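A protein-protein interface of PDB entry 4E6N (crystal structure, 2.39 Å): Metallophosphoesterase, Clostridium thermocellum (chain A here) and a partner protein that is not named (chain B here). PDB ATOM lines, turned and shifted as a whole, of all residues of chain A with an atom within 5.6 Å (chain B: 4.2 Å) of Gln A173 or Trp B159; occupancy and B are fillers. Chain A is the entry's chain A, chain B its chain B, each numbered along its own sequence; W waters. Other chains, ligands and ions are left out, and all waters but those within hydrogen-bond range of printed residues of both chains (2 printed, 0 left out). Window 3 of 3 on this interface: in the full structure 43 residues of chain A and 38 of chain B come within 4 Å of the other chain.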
ATOM      1  N   TRP A 168      30.321 -10.057 -21.828  1.00  0.00           N
ATOM      2  CA  TRP A 168      29.636 -11.029 -20.979  1.00  0.00           C
ATOM      3  C   TRP A 168      28.858 -10.359 -19.848  1.00  0.00           C
ATOM      4  O   TRP A 168      27.709 -10.703 -19.570  1.00  0.00           O
ATOM      5  CB  TRP A 168      30.694 -11.948 -20.374  1.00  0.00           C
ATOM      6  CG  TRP A 168      30.183 -13.065 -19.527  1.00  0.00           C
ATOM      7  CD1 TRP A 168      29.093 -13.847 -19.761  1.00  0.00           C
ATOM      8  CD2 TRP A 168      30.753 -13.523 -18.297  1.00  0.00           C
ATOM      9  NE1 TRP A 168      28.956 -14.778 -18.759  1.00  0.00           N
ATOM     10  CE2 TRP A 168      29.963 -14.596 -17.844  1.00  0.00           C
ATOM     11  CE3 TRP A 168      31.872 -13.144 -17.549  1.00  0.00           C
ATOM     12  CZ2 TRP A 168      30.250 -15.290 -16.672  1.00  0.00           C
ATOM     13  CZ3 TRP A 168      32.160 -13.824 -16.391  1.00  0.00           C
ATOM     14  CH2 TRP A 168      31.354 -14.890 -15.959  1.00  0.00           C
ATOM     15  N   SER A 169      29.503  -9.404 -19.185  1.00  0.00           N
ATOM     16  CA  SER A 169      28.902  -8.728 -18.039  1.00  0.00           C
ATOM     17  C   SER A 169      27.612  -7.989 -18.381  1.00  0.00           C
ATOM     18  O   SER A 169      26.836  -7.670 -17.499  1.00  0.00           O
ATOM     19  CB  SER A 169      29.901  -7.772 -17.380  1.00  0.00           C
ATOM     20  OG  SER A 169      30.424  -6.858 -18.317  1.00  0.00           O
ATOM     21  N   ALA A 170      27.372  -7.741 -19.660  1.00  0.00           N
ATOM     22  CA  ALA A 170      26.115  -7.125 -20.067  1.00  0.00           C
ATOM     23  C   ALA A 170      24.901  -8.013 -19.753  1.00  0.00           C
ATOM     24  O   ALA A 170      23.804  -7.504 -19.548  1.00  0.00           O
ATOM     25  CB  ALA A 170      26.148  -6.733 -21.560  1.00  0.00           C
ATOM     26  N   LYS A 171      25.091  -9.332 -19.717  1.00  0.00           N
ATOM     27  CA  LYS A 171      23.979 -10.242 -19.412  1.00  0.00           C
ATOM     28  C   LYS A 171      24.160 -11.012 -18.109  1.00  0.00           C
ATOM     29  O   LYS A 171      23.197 -11.535 -17.559  1.00  0.00           O
ATOM     30  CB  LYS A 171      23.753 -11.244 -20.549  1.00  0.00           C
ATOM     31  CG  LYS A 171      23.199 -10.613 -21.799  1.00  0.00           C
ATOM     32  CD  LYS A 171      21.749 -10.187 -21.602  1.00  0.00           C
ATOM     33  CE  LYS A 171      20.822 -11.395 -21.434  1.00  0.00           C
ATOM     34  NZ  LYS A 171      19.392 -10.983 -21.551  1.00  0.00           N
ATOM     35  N   ALA A 172      25.392 -11.064 -17.621  1.00  0.00           N
ATOM     36  CA  ALA A 172      25.745 -11.962 -16.528  1.00  0.00           C
ATOM     37  C   ALA A 172      25.968 -11.266 -15.185  1.00  0.00           C
ATOM     38  O   ALA A 172      26.461 -11.885 -14.243  1.00  0.00           O
ATOM     39  CB  ALA A 172      26.982 -12.790 -16.919  1.00  0.00           C
ATOM     40  N   GLN A 173      25.598  -9.993 -15.093  1.00  0.00           N
ATOM     41  CA  GLN A 173      25.893  -9.198 -13.895  1.00  0.00           C
ATOM     42  C   GLN A 173      25.391  -9.802 -12.571  1.00  0.00           C
ATOM     43  O   GLN A 173      26.084  -9.740 -11.546  1.00  0.00           O
ATOM     44  CB  GLN A 173      25.403  -7.748 -14.033  1.00  0.00           C
ATOM     45  CG  GLN A 173      25.850  -6.905 -12.860  1.00  0.00           C
ATOM     46  CD  GLN A 173      25.794  -5.430 -13.126  1.00  0.00           C
ATOM     47  OE1 GLN A 173      25.935  -4.989 -14.269  1.00  0.00           O
ATOM     48  NE2 GLN A 173      25.591  -4.645 -12.067  1.00  0.00           N
ATOM     49  N   LYS A 174      24.199 -10.389 -12.594  1.00  0.00           N
ATOM     50  CA  LYS A 174      23.667 -11.043 -11.403  1.00  0.00           C
ATOM     51  C   LYS A 174      24.531 -12.248 -11.006  1.00  0.00           C
ATOM     52  O   LYS A 174      24.777 -12.473  -9.821  1.00  0.00           O
ATOM     53  CB  LYS A 174      22.204 -11.448 -11.606  1.00  0.00           C
ATOM     54  CG  LYS A 174      21.619 -12.260 -10.461  1.00  0.00           C
ATOM     55  CD  LYS A 174      20.130 -12.534 -10.664  1.00  0.00           C
ATOM     56  CE  LYS A 174      19.256 -11.375 -10.176  1.00  0.00           C
ATOM     57  NZ  LYS A 174      19.393 -10.112 -10.974  1.00  0.00           N
ATOM     58  N   LEU A 175      24.998 -13.007 -11.995  1.00  0.00           N
ATOM     59  CA  LEU A 175      25.940 -14.098 -11.731  1.00  0.00           C
ATOM     60  C   LEU A 175      27.274 -13.581 -11.176  1.00  0.00           C
ATOM     61  O   LEU A 175      27.829 -14.156 -10.237  1.00  0.00           O
ATOM     62  CB  LEU A 175      26.193 -14.914 -12.991  1.00  0.00           C
ATOM     63  CG  LEU A 175      24.966 -15.616 -13.567  1.00  0.00           C
ATOM     64  CD1 LEU A 175      25.374 -16.525 -14.712  1.00  0.00           C
ATOM     65  CD2 LEU A 175      24.252 -16.407 -12.486  1.00  0.00           C
ATOM     66  N   LEU A 176      27.782 -12.500 -11.757  1.00  0.00           N
ATOM     67  CA  LEU A 176      29.036 -11.918 -11.306  1.00  0.00           C
ATOM     68  C   LEU A 176      28.908 -11.414  -9.870  1.00  0.00           C
ATOM     69  O   LEU A 176      29.800 -11.611  -9.051  1.00  0.00           O
ATOM     70  CB  LEU A 176      29.487 -10.798 -12.250  1.00  0.00           C
ATOM     71  CG  LEU A 176      30.059 -11.295 -13.592  1.00  0.00           C
ATOM     72  CD1 LEU A 176      29.873 -10.258 -14.699  1.00  0.00           C
ATOM     73  CD2 LEU A 176      31.537 -11.680 -13.472  1.00  0.00           C
ATOM     74  N   GLU A 177      27.776 -10.801  -9.557  1.00  0.00           N
ATOM     75  CA  GLU A 177      27.573 -10.251  -8.224  1.00  0.00           C
ATOM     76  C   GLU A 177      27.387 -11.337  -7.188  1.00  0.00           C
ATOM     77  O   GLU A 177      27.986 -11.283  -6.105  1.00  0.00           O
ATOM     78  CB  GLU A 177      26.349  -9.339  -8.172  1.00  0.00           C
ATOM     79  CG  GLU A 177      26.470  -8.050  -8.933  1.00  0.00           C
ATOM     80  CD  GLU A 177      25.201  -7.246  -8.826  1.00  0.00           C
ATOM     81  OE1 GLU A 177      24.244  -7.779  -8.224  1.00  0.00           O
ATOM     82  OE2 GLU A 177      25.160  -6.099  -9.324  1.00  0.00           O
ATOM     83  N   GLU A 178      26.549 -12.312  -7.509  1.00  0.00           N
ATOM     84  CA  GLU A 178      26.148 -13.297  -6.508  1.00  0.00           C
ATOM     85  C   GLU A 178      27.055 -14.510  -6.425  1.00  0.00           C
ATOM     86  O   GLU A 178      27.055 -15.208  -5.419  1.00  0.00           O
ATOM     87  CB  GLU A 178      24.710 -13.747  -6.739  1.00  0.00           C
ATOM     88  CG  GLU A 178      23.718 -12.596  -6.715  1.00  0.00           C
ATOM     89  CD  GLU A 178      22.304 -13.033  -7.048  1.00  0.00           C
ATOM     90  OE1 GLU A 178      21.420 -12.154  -7.120  1.00  0.00           O
ATOM     91  OE2 GLU A 178      22.077 -14.251  -7.240  1.00  0.00           O
ATOM     92  N   SER A 181      32.178 -12.840  -8.178  1.00  0.00           N
ATOM     93  CA  SER A 181      32.916 -11.866  -7.390  1.00  0.00           C
ATOM     94  C   SER A 181      32.811 -12.168  -5.889  1.00  0.00           C
ATOM     95  O   SER A 181      33.594 -11.668  -5.097  1.00  0.00           O
ATOM     96  CB  SER A 181      32.402 -10.459  -7.670  1.00  0.00           C
ATOM     97  OG  SER A 181      31.115 -10.293  -7.106  1.00  0.00           O
ATOM     98  N   TYR A 243      38.052 -13.667 -14.653  1.00  0.00           N
ATOM     99  CA  TYR A 243      36.678 -13.220 -14.861  1.00  0.00           C
ATOM    100  C   TYR A 243      36.591 -11.744 -15.230  1.00  0.00           C
ATOM    101  O   TYR A 243      35.674 -11.346 -15.960  1.00  0.00           O
ATOM    102  CB  TYR A 243      35.716 -13.591 -13.705  1.00  0.00           C
ATOM    103  CG  TYR A 243      35.746 -12.713 -12.451  1.00  0.00           C
ATOM    104  CD1 TYR A 243      35.314 -11.384 -12.482  1.00  0.00           C
ATOM    105  CD2 TYR A 243      36.138 -13.243 -11.213  1.00  0.00           C
ATOM    106  CE1 TYR A 243      35.331 -10.600 -11.351  1.00  0.00           C
ATOM    107  CE2 TYR A 243      36.143 -12.461 -10.065  1.00  0.00           C
ATOM    108  CZ  TYR A 243      35.745 -11.139 -10.138  1.00  0.00           C
ATOM    109  OH  TYR A 243      35.742 -10.350  -9.002  1.00  0.00           O
ATOM    110  N   CYS A 247      34.508  -8.439 -18.452  1.00  0.00           N
ATOM    111  CA  CYS A 247      33.588  -7.462 -17.887  1.00  0.00           C
ATOM    112  C   CYS A 247      34.066  -6.043 -18.176  1.00  0.00           C
ATOM    113  O   CYS A 247      35.265  -5.741 -18.103  1.00  0.00           O
ATOM    114  CB  CYS A 247      33.467  -7.649 -16.374  1.00  0.00           C
ATOM    115  SG  CYS A 247      33.142  -9.327 -15.824  1.00  0.00           S
ATOM    116  N   LEU B 152      32.301  -6.375  -3.265  1.00  0.00           N
ATOM    117  CA  LEU B 152      32.489  -7.572  -4.089  1.00  0.00           C
ATOM    118  C   LEU B 152      33.732  -7.475  -4.949  1.00  0.00           C
ATOM    119  O   LEU B 152      34.491  -8.434  -5.063  1.00  0.00           O
ATOM    120  CB  LEU B 152      31.273  -7.818  -4.965  1.00  0.00           C
ATOM    121  CG  LEU B 152      30.109  -8.392  -4.167  1.00  0.00           C
ATOM    122  CD1 LEU B 152      28.791  -8.172  -4.884  1.00  0.00           C
ATOM    123  CD2 LEU B 152      30.374  -9.871  -3.929  1.00  0.00           C
ATOM    124  N   ASP B 153      33.947  -6.311  -5.541  1.00  0.00           N
ATOM    125  CA  ASP B 153      35.105  -6.117  -6.397  1.00  0.00           C
ATOM    126  C   ASP B 153      35.402  -4.638  -6.524  1.00  0.00           C
ATOM    127  O   ASP B 153      34.616  -3.886  -7.108  1.00  0.00           O
ATOM    128  CB  ASP B 153      34.884  -6.729  -7.787  1.00  0.00           C
ATOM    129  CG  ASP B 153      36.171  -6.821  -8.602  1.00  0.00           C
ATOM    130  OD1 ASP B 153      36.993  -5.881  -8.569  1.00  0.00           O
ATOM    131  OD2 ASP B 153      36.366  -7.838  -9.292  1.00  0.00           O
ATOM    132  N   PHE B 156      34.966  -2.922  -9.673  1.00  0.00           N
ATOM    133  CA  PHE B 156      33.566  -2.768 -10.068  1.00  0.00           C
ATOM    134  C   PHE B 156      32.648  -2.376  -8.905  1.00  0.00           C
ATOM    135  O   PHE B 156      31.769  -3.154  -8.508  1.00  0.00           O
ATOM    136  CB  PHE B 156      33.050  -4.055 -10.728  1.00  0.00           C
ATOM    137  CG  PHE B 156      33.677  -4.333 -12.049  1.00  0.00           C
ATOM    138  CD1 PHE B 156      33.107  -3.846 -13.212  1.00  0.00           C
ATOM    139  CD2 PHE B 156      34.864  -5.054 -12.125  1.00  0.00           C
ATOM    140  CE1 PHE B 156      33.707  -4.089 -14.438  1.00  0.00           C
ATOM    141  CE2 PHE B 156      35.474  -5.290 -13.337  1.00  0.00           C
ATOM    142  CZ  PHE B 156      34.900  -4.813 -14.499  1.00  0.00           C
ATOM    143  N   PRO B 157      32.831  -1.154  -8.370  1.00  0.00           N
ATOM    144  CA  PRO B 157      32.047  -0.710  -7.208  1.00  0.00           C
ATOM    145  C   PRO B 157      30.534  -0.717  -7.466  1.00  0.00           C
ATOM    146  O   PRO B 157      29.735  -0.811  -6.533  1.00  0.00           O
ATOM    147  CB  PRO B 157      32.560   0.716  -6.960  1.00  0.00           C
ATOM    148  CG  PRO B 157      33.180   1.147  -8.283  1.00  0.00           C
ATOM    149  CD  PRO B 157      33.775  -0.119  -8.834  1.00  0.00           C
ATOM    150  N   GLU B 158      30.153  -0.624  -8.732  1.00  0.00           N
ATOM    151  CA  GLU B 158      28.751  -0.732  -9.130  1.00  0.00           C
ATOM    152  C   GLU B 158      28.109  -2.092  -8.805  1.00  0.00           C
ATOM    153  O   GLU B 158      26.889  -2.183  -8.684  1.00  0.00           O
ATOM    154  CB  GLU B 158      28.590  -0.414 -10.624  1.00  0.00           C
ATOM    155  CG  GLU B 158      29.445  -1.274 -11.555  1.00  0.00           C
ATOM    156  CD  GLU B 158      30.833  -0.706 -11.768  1.00  0.00           C
ATOM    157  OE1 GLU B 158      31.359  -0.061 -10.840  1.00  0.00           O
ATOM    158  OE2 GLU B 158      31.399  -0.889 -12.872  1.00  0.00           O
ATOM    159  N   TRP B 159      28.913  -3.147  -8.666  1.00  0.00           N
ATOM    160  CA  TRP B 159      28.353  -4.440  -8.260  1.00  0.00           C
ATOM    161  C   TRP B 159      27.913  -4.421  -6.802  1.00  0.00           C
ATOM    162  O   TRP B 159      27.189  -5.314  -6.355  1.00  0.00           O
ATOM    163  CB  TRP B 159      29.331  -5.591  -8.483  1.00  0.00           C
ATOM    164  CG  TRP B 159      29.652  -5.841  -9.906  1.00  0.00           C
ATOM    165  CD1 TRP B 159      28.992  -5.353 -10.998  1.00  0.00           C
ATOM    166  CD2 TRP B 159      30.731  -6.626 -10.406  1.00  0.00           C
ATOM    167  NE1 TRP B 159      29.599  -5.785 -12.144  1.00  0.00           N
ATOM    168  CE2 TRP B 159      30.671  -6.570 -11.811  1.00  0.00           C
ATOM    169  CE3 TRP B 159      31.746  -7.371  -9.803  1.00  0.00           C
ATOM    170  CZ2 TRP B 159      31.584  -7.241 -12.627  1.00  0.00           C
ATOM    171  CZ3 TRP B 159      32.658  -8.035 -10.618  1.00  0.00           C
ATOM    172  CH2 TRP B 159      32.569  -7.965 -12.012  1.00  0.00           C
ATOM    173  N   GLY B 160      28.361  -3.412  -6.064  1.00  0.00           N
ATOM    174  CA  GLY B 160      27.961  -3.252  -4.669  1.00  0.00           C
ATOM    175  C   GLY B 160      28.757  -4.052  -3.645  1.00  0.00           C
ATOM    176  O   GLY B 160      29.814  -4.614  -3.946  1.00  0.00           O
HETATM  177  O   HOH W   1      28.699  -5.162 -15.267  1.00  0.00           O
HETATM  178  O   HOH W   2      36.527 -10.220  -6.124  1.00  0.00           O
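Gln A173 touches just one residue of chain B: Trp B159 (3.6 Å).
Printed residues of chain B within 4 Å of Glu A177: Leu B152 (3.4 Å) and Trp B159 (3.7 Å).
Glu A178 touches none of the printed residues of chain B.
Of the printed residues of chain B, Tyr A243 touches Asp B153 (2.6 Å) and Trp B159 (3.8 Å).
Printed residues of chain B within 4 Å of Cys A247: Phe B156.
Of the printed residues of chain A, Asp B153 touches Tyr A243 (2.6 Å).
Trp B159 touches four residues of chain A.
Gly B160 touches none of the printed residues of chain A.
The nearest printed residue of chain B that does not touch Gln A173 is Glu B158 (4.4 Å).
The nearest printed residue of chain A that does not touch Leu B152 is Tyr A243 (4.6 Å).
Water W2 lies within hydrogen-bond range of O of Leu B152 (2.9 Å), OH of Tyr A243 (3.0 Å) and O of Ser A181 (3.4 Å).
Water W1 lies within hydrogen-bond range of OE1 of Gln A173 (2.9 Å) and NE1 of Trp B159 (3.3 Å).
Among the printed residues, pairs that only touch across the chains: Gln A173 with Trp B159, Glu A177 with Leu B152, Glu A177 with Trp B159, Ser A181 with Trp B159, Tyr A243 with Trp B159 and Cys A247 with Phe B156.
O of Gly B160 sits at hydrogen-bond distance from N of Leu B152, 3.1 Å away.
O of Leu A176 lies within hydrogen-bond range of OG of Ser A181, 2.7 Å away.
OG of Ser A181 sits at hydrogen-bond distance from O of Glu A177 (3.4 Å).
NE2 of Gln A173 lies within hydrogen-bond range of OE2 of Glu A177.
O of Tyr A243 sits at hydrogen-bond distance from SG of Cys A247 (3.2 Å).
Printed residues of chain A that touch a printed residue of chain B: Gln A173, Glu A177, Ser A181, Tyr A243 and Cys A247.
The backbone carbonyl oxygen (O) of Ser A181 lies close to the backbone carbonyl oxygen (O) of Leu B152 (3.4 Å).
OD2 of Asp B153 is in hydrogen-bond range of OH of Tyr A243 (2.6 Å).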
